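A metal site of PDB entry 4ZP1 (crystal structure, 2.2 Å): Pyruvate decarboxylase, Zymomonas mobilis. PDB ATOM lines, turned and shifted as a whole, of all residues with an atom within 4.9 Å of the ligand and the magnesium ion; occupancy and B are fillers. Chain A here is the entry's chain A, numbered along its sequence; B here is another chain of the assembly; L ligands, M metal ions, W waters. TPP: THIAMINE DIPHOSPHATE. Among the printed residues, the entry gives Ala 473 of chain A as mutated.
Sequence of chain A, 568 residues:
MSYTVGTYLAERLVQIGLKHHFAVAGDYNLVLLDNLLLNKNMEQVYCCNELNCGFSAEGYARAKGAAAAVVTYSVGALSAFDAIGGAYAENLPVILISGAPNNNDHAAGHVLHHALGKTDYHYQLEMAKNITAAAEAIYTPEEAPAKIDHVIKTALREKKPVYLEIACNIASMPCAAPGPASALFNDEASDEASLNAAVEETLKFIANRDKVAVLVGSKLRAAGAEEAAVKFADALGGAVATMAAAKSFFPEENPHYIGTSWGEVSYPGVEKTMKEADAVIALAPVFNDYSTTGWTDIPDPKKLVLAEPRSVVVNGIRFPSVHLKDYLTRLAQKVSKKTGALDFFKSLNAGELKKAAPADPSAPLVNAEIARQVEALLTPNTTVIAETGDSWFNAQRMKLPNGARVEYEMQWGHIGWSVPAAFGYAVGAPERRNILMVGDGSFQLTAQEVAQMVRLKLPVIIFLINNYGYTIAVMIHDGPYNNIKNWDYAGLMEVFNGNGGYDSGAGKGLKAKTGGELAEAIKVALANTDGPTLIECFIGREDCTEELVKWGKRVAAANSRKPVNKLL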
ATOM      1  N   THR A 388      -2.396  16.370 -31.003  1.00  0.00           N
ATOM      2  CA  THR A 388      -2.963  15.923 -29.738  1.00  0.00           C
ATOM      3  C   THR A 388      -1.964  15.070 -28.956  1.00  0.00           C
ATOM      4  O   THR A 388      -1.440  14.083 -29.462  1.00  0.00           O
ATOM      5  CB  THR A 388      -4.239  15.077 -29.966  1.00  0.00           C
ATOM      6  OG1 THR A 388      -5.256  15.888 -30.586  1.00  0.00           O
ATOM      7  CG2 THR A 388      -4.759  14.515 -28.654  1.00  0.00           C
ATOM      8  N   GLY A 389      -1.719  15.470 -27.706  1.00  0.00           N
ATOM      9  CA  GLY A 389      -0.710  14.848 -26.876  1.00  0.00           C
ATOM     10  C   GLY A 389      -0.014  15.948 -26.099  1.00  0.00           C
ATOM     11  O   GLY A 389      -0.496  17.096 -26.098  1.00  0.00           O
ATOM     12  N   ASP A 390       1.115  15.644 -25.464  1.00  0.00           N
ATOM     13  CA  ASP A 390       1.847  16.665 -24.716  1.00  0.00           C
ATOM     14  C   ASP A 390       2.274  17.811 -25.641  1.00  0.00           C
ATOM     15  O   ASP A 390       2.546  18.919 -25.183  1.00  0.00           O
ATOM     16  CB  ASP A 390       3.065  16.091 -24.018  1.00  0.00           C
ATOM     17  CG  ASP A 390       3.562  16.984 -22.886  1.00  0.00           C
ATOM     18  OD1 ASP A 390       2.722  17.679 -22.274  1.00  0.00           O
ATOM     19  OD2 ASP A 390       4.779  16.992 -22.605  1.00  0.00           O
ATOM     20  N   GLY A 413      -9.757  16.195 -32.116  1.00  0.00           N
ATOM     21  CA  GLY A 413      -8.755  15.501 -31.323  1.00  0.00           C
ATOM     22  C   GLY A 413      -8.349  14.138 -31.868  1.00  0.00           C
ATOM     23  O   GLY A 413      -8.164  13.202 -31.094  1.00  0.00           O
ATOM     24  N   HIS A 414      -8.203  14.047 -33.184  1.00  0.00           N
ATOM     25  CA  HIS A 414      -7.869  12.783 -33.834  1.00  0.00           C
ATOM     26  C   HIS A 414      -6.371  12.592 -33.910  1.00  0.00           C
ATOM     27  O   HIS A 414      -5.702  13.298 -34.661  1.00  0.00           O
ATOM     28  CB  HIS A 414      -8.481  12.749 -35.241  1.00  0.00           C
ATOM     29  CG  HIS A 414      -8.410  11.410 -35.902  1.00  0.00           C
ATOM     30  ND1 HIS A 414      -7.224  10.850 -36.339  1.00  0.00           N
ATOM     31  CD2 HIS A 414      -9.379  10.511 -36.201  1.00  0.00           C
ATOM     32  CE1 HIS A 414      -7.479   9.671 -36.877  1.00  0.00           C
ATOM     33  NE2 HIS A 414      -8.777   9.444 -36.811  1.00  0.00           N
ATOM     34  N   ILE A 415      -5.812  11.653 -33.150  1.00  0.00           N
ATOM     35  CA  ILE A 415      -4.367  11.468 -33.223  1.00  0.00           C
ATOM     36  C   ILE A 415      -3.998  11.055 -34.642  1.00  0.00           C
ATOM     37  O   ILE A 415      -4.747  10.317 -35.298  1.00  0.00           O
ATOM     38  CB  ILE A 415      -3.840  10.438 -32.197  1.00  0.00           C
ATOM     39  CG1 ILE A 415      -4.238   9.014 -32.573  1.00  0.00           C
ATOM     40  CG2 ILE A 415      -4.328  10.773 -30.793  1.00  0.00           C
ATOM     41  CD1 ILE A 415      -3.609   7.973 -31.657  1.00  0.00           C
ATOM     42  N   GLY A 439       3.784  13.256 -31.573  1.00  0.00           N
ATOM     43  CA  GLY A 439       4.247  12.167 -30.734  1.00  0.00           C
ATOM     44  C   GLY A 439       4.343  10.868 -31.508  1.00  0.00           C
ATOM     45  O   GLY A 439       3.718  10.721 -32.556  1.00  0.00           O
ATOM     46  N   ASP A 440       5.121   9.921 -30.983  1.00  0.00           N
ATOM     47  CA  ASP A 440       5.324   8.655 -31.681  1.00  0.00           C
ATOM     48  C   ASP A 440       4.006   7.904 -31.892  1.00  0.00           C
ATOM     49  O   ASP A 440       3.774   7.347 -32.970  1.00  0.00           O
ATOM     50  CB  ASP A 440       6.320   7.767 -30.912  1.00  0.00           C
ATOM     51  CG  ASP A 440       5.927   7.559 -29.454  1.00  0.00           C
ATOM     52  OD1 ASP A 440       5.179   8.386 -28.906  1.00  0.00           O
ATOM     53  OD2 ASP A 440       6.384   6.567 -28.848  1.00  0.00           O
ATOM     54  N   GLY A 441       3.149   7.913 -30.881  1.00  0.00           N
ATOM     55  CA  GLY A 441       1.878   7.219 -30.955  1.00  0.00           C
ATOM     56  C   GLY A 441       0.995   7.699 -32.097  1.00  0.00           C
ATOM     57  O   GLY A 441       0.458   6.889 -32.852  1.00  0.00           O
ATOM     58  N   SER A 442       0.859   9.019 -32.213  1.00  0.00           N
ATOM     59  CA  SER A 442       0.023   9.612 -33.258  1.00  0.00           C
ATOM     60  C   SER A 442       0.635   9.422 -34.630  1.00  0.00           C
ATOM     61  O   SER A 442      -0.077   9.197 -35.623  1.00  0.00           O
ATOM     62  CB  SER A 442      -0.186  11.113 -32.982  1.00  0.00           C
ATOM     63  OG  SER A 442      -0.632  11.320 -31.660  1.00  0.00           O
ATOM     64  N   PHE A 443       1.963   9.531 -34.696  1.00  0.00           N
ATOM     65  CA  PHE A 443       2.681   9.473 -35.960  1.00  0.00           C
ATOM     66  C   PHE A 443       2.441   8.131 -36.684  1.00  0.00           C
ATOM     67  O   PHE A 443       2.451   8.090 -37.914  1.00  0.00           O
ATOM     68  CB  PHE A 443       4.178   9.698 -35.738  1.00  0.00           C
ATOM     69  CG  PHE A 443       5.014   9.704 -37.005  1.00  0.00           C
ATOM     70  CD1 PHE A 443       5.205  10.869 -37.726  1.00  0.00           C
ATOM     71  CD2 PHE A 443       5.613   8.535 -37.463  1.00  0.00           C
ATOM     72  CE1 PHE A 443       5.975  10.874 -38.884  1.00  0.00           C
ATOM     73  CE2 PHE A 443       6.385   8.530 -38.620  1.00  0.00           C
ATOM     74  CZ  PHE A 443       6.567   9.695 -39.330  1.00  0.00           C
ATOM     75  N   LEU A 445      -0.241   6.395 -36.975  1.00  0.00           N
ATOM     76  CA  LEU A 445      -1.533   6.260 -37.644  1.00  0.00           C
ATOM     77  C   LEU A 445      -1.518   6.719 -39.103  1.00  0.00           C
ATOM     78  O   LEU A 445      -2.293   6.231 -39.917  1.00  0.00           O
ATOM     79  CB  LEU A 445      -2.618   7.045 -36.902  1.00  0.00           C
ATOM     80  CG  LEU A 445      -3.302   6.365 -35.705  1.00  0.00           C
ATOM     81  CD1 LEU A 445      -2.446   6.496 -34.452  1.00  0.00           C
ATOM     82  CD2 LEU A 445      -4.700   6.933 -35.496  1.00  0.00           C
ATOM     83  N   ILE A 465       8.440  13.194 -31.127  1.00  0.00           N
ATOM     84  CA  ILE A 465       8.712  12.934 -29.713  1.00  0.00           C
ATOM     85  C   ILE A 465       8.608  11.443 -29.398  1.00  0.00           C
ATOM     86  O   ILE A 465       7.508  10.924 -29.204  1.00  0.00           O
ATOM     87  CB  ILE A 465       7.747  13.704 -28.817  1.00  0.00           C
ATOM     88  CG1 ILE A 465       7.610  15.142 -29.303  1.00  0.00           C
ATOM     89  CG2 ILE A 465       8.233  13.676 -27.385  1.00  0.00           C
ATOM     90  CD1 ILE A 465       8.926  15.883 -29.345  1.00  0.00           C
ATOM     91  N   ASN A 467       8.721   9.062 -26.859  1.00  0.00           N
ATOM     92  CA  ASN A 467       8.672   8.756 -25.436  1.00  0.00           C
ATOM     93  C   ASN A 467       8.175   7.329 -25.208  1.00  0.00           C
ATOM     94  O   ASN A 467       7.920   6.929 -24.074  1.00  0.00           O
ATOM     95  CB  ASN A 467       7.769   9.757 -24.712  1.00  0.00           C
ATOM     96  CG  ASN A 467       6.379   9.836 -25.320  1.00  0.00           C
ATOM     97  OD1 ASN A 467       5.965   8.927 -26.048  1.00  0.00           O
ATOM     98  ND2 ASN A 467       5.662  10.921 -25.039  1.00  0.00           N
ATOM     99  N   TYR A 468       8.008   6.587 -26.308  1.00  0.00           N
ATOM    100  CA  TYR A 468       7.644   5.174 -26.290  1.00  0.00           C
ATOM    101  C   TYR A 468       6.269   4.869 -25.671  1.00  0.00           C
ATOM    102  O   TYR A 468       6.182   4.074 -24.724  1.00  0.00           O
ATOM    103  CB  TYR A 468       8.744   4.381 -25.569  1.00  0.00           C
ATOM    104  CG  TYR A 468       8.660   2.883 -25.776  1.00  0.00           C
ATOM    105  CD1 TYR A 468       8.434   2.359 -27.045  1.00  0.00           C
ATOM    106  CD2 TYR A 468       8.800   2.003 -24.712  1.00  0.00           C
ATOM    107  CE1 TYR A 468       8.360   0.991 -27.248  1.00  0.00           C
ATOM    108  CE2 TYR A 468       8.729   0.625 -24.913  1.00  0.00           C
ATOM    109  CZ  TYR A 468       8.505   0.134 -26.178  1.00  0.00           C
ATOM    110  OH  TYR A 468       8.427  -1.226 -26.392  1.00  0.00           O
ATOM    111  N   GLY A 469       5.213   5.475 -26.197  1.00  0.00           N
ATOM    112  CA  GLY A 469       3.857   5.156 -25.761  1.00  0.00           C
ATOM    113  C   GLY A 469       2.878   6.317 -25.786  1.00  0.00           C
ATOM    114  O   GLY A 469       3.265   7.452 -26.070  1.00  0.00           O
ATOM    115  N   TYR A 470       1.605   6.041 -25.489  1.00  0.00           N
ATOM    116  CA  TYR A 470       0.560   7.076 -25.402  1.00  0.00           C
ATOM    117  C   TYR A 470       0.614   7.827 -24.058  1.00  0.00           C
ATOM    118  O   TYR A 470      -0.196   7.547 -23.160  1.00  0.00           O
ATOM    119  CB  TYR A 470      -0.840   6.469 -25.561  1.00  0.00           C
ATOM    120  CG  TYR A 470      -1.133   5.743 -26.857  1.00  0.00           C
ATOM    121  CD1 TYR A 470      -0.465   6.053 -28.033  1.00  0.00           C
ATOM    122  CD2 TYR A 470      -2.101   4.739 -26.900  1.00  0.00           C
ATOM    123  CE1 TYR A 470      -0.755   5.378 -29.216  1.00  0.00           C
ATOM    124  CE2 TYR A 470      -2.390   4.066 -28.074  1.00  0.00           C
ATOM    125  CZ  TYR A 470      -1.711   4.382 -29.232  1.00  0.00           C
ATOM    126  OH  TYR A 470      -2.006   3.699 -30.392  1.00  0.00           O
ATOM    127  N   THR A 471       1.538   8.772 -23.917  1.00  0.00           N
ATOM    128  CA  THR A 471       1.808   9.386 -22.619  1.00  0.00           C
ATOM    129  C   THR A 471       0.624  10.206 -22.069  1.00  0.00           C
ATOM    130  O   THR A 471       0.349  10.168 -20.870  1.00  0.00           O
ATOM    131  CB  THR A 471       3.060  10.285 -22.675  1.00  0.00           C
ATOM    132  OG1 THR A 471       4.232   9.455 -22.751  1.00  0.00           O
ATOM    133  CG2 THR A 471       3.162  11.159 -21.430  1.00  0.00           C
ATOM    134  N   ILE A 472      -0.056  10.945 -22.942  1.00  0.00           N
ATOM    135  CA  ILE A 472      -1.228  11.726 -22.519  1.00  0.00           C
ATOM    136  C   ILE A 472      -2.316  10.783 -21.989  1.00  0.00           C
ATOM    137  O   ILE A 472      -3.040  11.122 -21.054  1.00  0.00           O
ATOM    138  CB  ILE A 472      -1.794  12.601 -23.654  1.00  0.00           C
ATOM    139  CG1 ILE A 472      -3.111  13.258 -23.234  1.00  0.00           C
ATOM    140  CG2 ILE A 472      -1.992  11.772 -24.909  1.00  0.00           C
ATOM    141  CD1 ILE A 472      -3.572  14.362 -24.178  1.00  0.00           C
ATOM    142  N   ALA A 473      -2.414   9.605 -22.594  1.00  0.00           N
ATOM    143  CA  ALA A 473      -3.333   8.573 -22.125  1.00  0.00           C
ATOM    144  C   ALA A 473      -2.868   8.008 -20.784  1.00  0.00           C
ATOM    145  O   ALA A 473      -3.681   7.623 -19.947  1.00  0.00           O
ATOM    146  CB  ALA A 473      -3.480   7.468 -23.158  1.00  0.00           C
ATOM    147  N   VAL B  24      -8.039  -0.164 -30.233  1.00  0.00           N
ATOM    148  CA  VAL B  24      -7.259   1.051 -30.253  1.00  0.00           C
ATOM    149  C   VAL B  24      -7.721   1.866 -29.046  1.00  0.00           C
ATOM    150  O   VAL B  24      -8.891   2.245 -28.965  1.00  0.00           O
ATOM    151  CB  VAL B  24      -7.446   1.857 -31.555  1.00  0.00           C
ATOM    152  CG1 VAL B  24      -6.746   3.203 -31.470  1.00  0.00           C
ATOM    153  CG2 VAL B  24      -6.944   1.054 -32.759  1.00  0.00           C
ATOM    154  N   ALA B  25      -6.819   2.094 -28.102  1.00  0.00           N
ATOM    155  CA  ALA B  25      -7.202   2.778 -26.866  1.00  0.00           C
ATOM    156  C   ALA B  25      -7.633   4.234 -27.123  1.00  0.00           C
ATOM    157  O   ALA B  25      -7.173   4.885 -28.048  1.00  0.00           O
ATOM    158  CB  ALA B  25      -6.066   2.736 -25.863  1.00  0.00           C
ATOM    159  N   GLY B  26      -8.542   4.717 -26.280  1.00  0.00           N
ATOM    160  CA  GLY B  26      -9.016   6.076 -26.350  1.00  0.00           C
ATOM    161  C   GLY B  26      -9.649   6.412 -25.014  1.00  0.00           C
ATOM    162  O   GLY B  26     -10.094   5.499 -24.307  1.00  0.00           O
ATOM    163  N   ASP B  27      -9.727   7.690 -24.657  1.00  0.00           N
ATOM    164  CA  ASP B  27     -10.185   8.033 -23.319  1.00  0.00           C
ATOM    165  C   ASP B  27     -11.664   7.708 -23.095  1.00  0.00           C
ATOM    166  O   ASP B  27     -12.152   7.765 -21.975  1.00  0.00           O
ATOM    167  CB  ASP B  27      -9.916   9.515 -23.014  1.00  0.00           C
ATOM    168  CG  ASP B  27     -10.859  10.453 -23.757  1.00  0.00           C
ATOM    169  OD1 ASP B  27     -11.400  10.055 -24.816  1.00  0.00           O
ATOM    170  OD2 ASP B  27     -11.047  11.584 -23.270  1.00  0.00           O
ATOM    171  N   GLU B  50      -7.599   2.831 -36.511  1.00  0.00           N
ATOM    172  CA  GLU B  50      -8.882   2.150 -36.422  1.00  0.00           C
ATOM    173  C   GLU B  50      -9.300   1.462 -37.724  1.00  0.00           C
ATOM    174  O   GLU B  50      -9.996   0.451 -37.699  1.00  0.00           O
ATOM    175  CB  GLU B  50      -9.976   3.123 -35.992  1.00  0.00           C
ATOM    176  CG  GLU B  50      -9.819   3.643 -34.562  1.00  0.00           C
ATOM    177  CD  GLU B  50      -8.766   4.726 -34.440  1.00  0.00           C
ATOM    178  OE1 GLU B  50      -8.242   5.186 -35.478  1.00  0.00           O
ATOM    179  OE2 GLU B  50      -8.465   5.136 -33.289  1.00  0.00           O
ATOM    180  N   THR B  72     -12.651   4.054 -29.840  1.00  0.00           N
ATOM    181  CA  THR B  72     -13.178   5.142 -29.036  1.00  0.00           C
ATOM    182  C   THR B  72     -14.192   5.956 -29.840  1.00  0.00           C
ATOM    183  O   THR B  72     -14.339   5.770 -31.048  1.00  0.00           O
ATOM    184  CB  THR B  72     -12.041   6.040 -28.518  1.00  0.00           C
ATOM    185  OG1 THR B  72     -12.533   6.884 -27.466  1.00  0.00           O
ATOM    186  CG2 THR B  72     -11.462   6.892 -29.636  1.00  0.00           C
ATOM    187  N   VAL B  75     -13.821   9.694 -33.329  1.00  0.00           N
ATOM    188  CA  VAL B  75     -12.548   9.748 -34.024  1.00  0.00           C
ATOM    189  C   VAL B  75     -12.071   8.343 -34.364  1.00  0.00           C
ATOM    190  O   VAL B  75     -11.422   8.128 -35.377  1.00  0.00           O
ATOM    191  CB  VAL B  75     -11.470  10.481 -33.193  1.00  0.00           C
ATOM    192  CG1 VAL B  75     -11.821  11.958 -33.073  1.00  0.00           C
ATOM    193  CG2 VAL B  75     -11.336   9.838 -31.826  1.00  0.00           C
ATOM    194  N   GLY B  76     -12.412   7.388 -33.515  1.00  0.00           N
ATOM    195  CA  GLY B  76     -12.052   6.007 -33.767  1.00  0.00           C
ATOM    196  C   GLY B  76     -13.078   5.322 -34.652  1.00  0.00           C
ATOM    197  O   GLY B  76     -12.744   4.770 -35.704  1.00  0.00           O
ATOM    198  N   HIS B 114     -13.879  15.309 -29.251  1.00  0.00           N
ATOM    199  CA  HIS B 114     -14.093  14.178 -30.140  1.00  0.00           C
ATOM    200  C   HIS B 114     -15.482  14.158 -30.770  1.00  0.00           C
ATOM    201  O   HIS B 114     -15.871  13.157 -31.340  1.00  0.00           O
ATOM    202  CB  HIS B 114     -13.886  12.839 -29.424  1.00  0.00           C
ATOM    203  CG  HIS B 114     -12.474  12.566 -29.016  1.00  0.00           C
ATOM    204  ND1 HIS B 114     -11.395  13.266 -29.539  1.00  0.00           N
ATOM    205  CD2 HIS B 114     -11.943  11.667 -28.159  1.00  0.00           C
ATOM    206  CE1 HIS B 114     -10.285  12.813 -29.007  1.00  0.00           C
ATOM    207  NE2 HIS B 114     -10.582  11.849 -28.161  1.00  0.00           N
HETATM  208  N1' TPP L   1      -7.684   7.226 -31.748  1.00  0.00           N
HETATM  209  C2' TPP L   1      -7.870   8.389 -32.484  1.00  0.00           C
HETATM  210  CM2 TPP L   1      -8.132   8.293 -33.964  1.00  0.00           C
HETATM  211  N3' TPP L   1      -7.817   9.630 -31.867  1.00  0.00           N
HETATM  212  C4' TPP L   1      -7.581   9.719 -30.506  1.00  0.00           C
HETATM  213  N4' TPP L   1      -7.530  10.914 -29.910  1.00  0.00           N
HETATM  214  C5' TPP L   1      -7.393   8.560 -29.751  1.00  0.00           C
HETATM  215  C6' TPP L   1      -7.457   7.313 -30.386  1.00  0.00           C
HETATM  216  C7' TPP L   1      -7.139   8.613 -28.261  1.00  0.00           C
HETATM  217  N3  TPP L   1      -5.869   9.199 -27.881  1.00  0.00           N
HETATM  218  C2  TPP L   1      -5.712  10.504 -27.440  1.00  0.00           C
HETATM  219  S1  TPP L   1      -4.200  10.872 -27.072  1.00  0.00           S
HETATM  220  C5  TPP L   1      -3.673   9.412 -27.457  1.00  0.00           C
HETATM  221  C4  TPP L   1      -4.682   8.554 -27.882  1.00  0.00           C
HETATM  222  CM4 TPP L   1      -4.489   7.120 -28.302  1.00  0.00           C
HETATM  223  C6  TPP L   1      -2.182   9.186 -27.281  1.00  0.00           C
HETATM  224  C7  TPP L   1      -1.305   9.963 -28.269  1.00  0.00           C
HETATM  225  O7  TPP L   1      -0.034   9.334 -28.384  1.00  0.00           O
HETATM  226  PA  TPP L   1       1.334  10.144 -28.730  1.00  0.00           P
HETATM  227  O1A TPP L   1       1.351  10.607 -30.170  1.00  0.00           O
HETATM  228  O2A TPP L   1       2.545   9.277 -28.456  1.00  0.00           O
HETATM  229  O3A TPP L   1       1.255  11.420 -27.739  1.00  0.00           O
HETATM  230  PB  TPP L   1       2.101  11.606 -26.383  1.00  0.00           P
HETATM  231  O1B TPP L   1       1.146  12.043 -25.291  1.00  0.00           O
HETATM  232  O2B TPP L   1       3.141  12.686 -26.576  1.00  0.00           O
HETATM  233  O3B TPP L   1       2.776  10.306 -25.975  1.00  0.00           O
HETATM  234 MG    MG M   1       4.065   8.981 -27.410  1.00  0.00          MG
HETATM  235  O   HOH W   1       1.284  13.480 -30.292  1.00  0.00           O
HETATM  236  O   HOH W   2       2.671  14.814 -28.502  1.00  0.00           O
HETATM  237  O   HOH W   3       5.084  10.970 -27.795  1.00  0.00           O
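O1A of the ligand lies within hydrogen-bond range of N of Ser 442, at 2.6 Å. The side-chain hydroxyl of Ser 442 is in hydrogen-bond range of an oxygen (O1A) of the ligand, at 2.6 Å. N4' of the ligand lies within hydrogen-bond range of O of Gly 413. The side-chain carboxylate (OE2) of Glu 50 of chain B sits at hydrogen-bond distance from a nitrogen (N1') of the ligand. An oxygen (O1A) of the ligand is in hydrogen-bond range of the backbone NH (N) of Gly 441, at 3.3 Å. N of Thr 471 sits close to O3B of the ligand, at 2.8 Å. An oxygen (O1B) of the ligand is in hydrogen-bond range of the backbone NH (N) of Ile 472. The backbone NH of Ile 415 lies within hydrogen-bond range of a nitrogen (N3') of the ligand.
The backbone NH of Asp 440 is in hydrogen-bond range of the backbone carbonyl oxygen of Ile 465 (3.1 Å). N of Tyr 468 lies within hydrogen-bond range of OD2 of Asp 440 (3.0 Å). The side-chain hydroxyl (OG1) of Thr 471 lies within hydrogen-bond range of the side-chain amide nitrogen (ND2) of Asn 467, at 3.1 Å. O of Val 75 of chain B sits close to NE2 of His 414 (3.3 Å).
O of Gly 439 sits close to O1A of the ligand (3.4 Å). Merely in contact with the ligand: Gly 389 (3.7 Å), Asp 390 (3.6 Å), His 414 (3.1 Å), Leu 445 (3.997 Å), Tyr 470 (3.3 Å), Ala 25 of chain B (3.4 Å), Gly 26 of chain B (3.7 Å), Val 75 of chain B (3.5 Å) and His 114 of chain B (3.5 Å). Hydrophobic or aromatic side chains within 4 Å of the ligand: His 414, Ile 415, Leu 445, Tyr 470, Ile 472, Val 75 of chain B and His 114 of chain B. 20 residues have an atom within 4 Å of the ligand: Gly 389, Asp 390, Gly 413, His 414, Ile 415, Gly 439, Asp 440, Gly 441, Ser 442, Leu 445, Asn 467, Gly 469, Tyr 470, Thr 471, Ile 472, Ala 25 of chain B, Gly 26 of chain B, Glu 50 of chain B, Val 75 of chain B and His 114 of chain B.
Gly 441 touches the magnesium ion (N to MG, 3.7 Å).
The magnesium ion is bound by an oxygen (O2A) of the ligand, the side-chain carboxylate (OD1) of Asp 440, the backbone carbonyl oxygen (O) of Gly 469, water W3, the side-chain amide oxygen (OD1) of Asn 467 and an oxygen (O3B) of the ligand.
Water W3 lies within hydrogen-bond range of the backbone carbonyl oxygen (O) of Ile 465, the side-chain amide nitrogen (ND2) of Asn 467, an oxygen (O2B) of the ligand and the backbone NH (N) of Asp 440. Water W1 lies within hydrogen-bond range of N of Gly 439 (2.8 Å), O1A of the ligand (2.9 Å), O of Thr 388 (2.9 Å) and OG of Ser 442 (3.2 Å).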
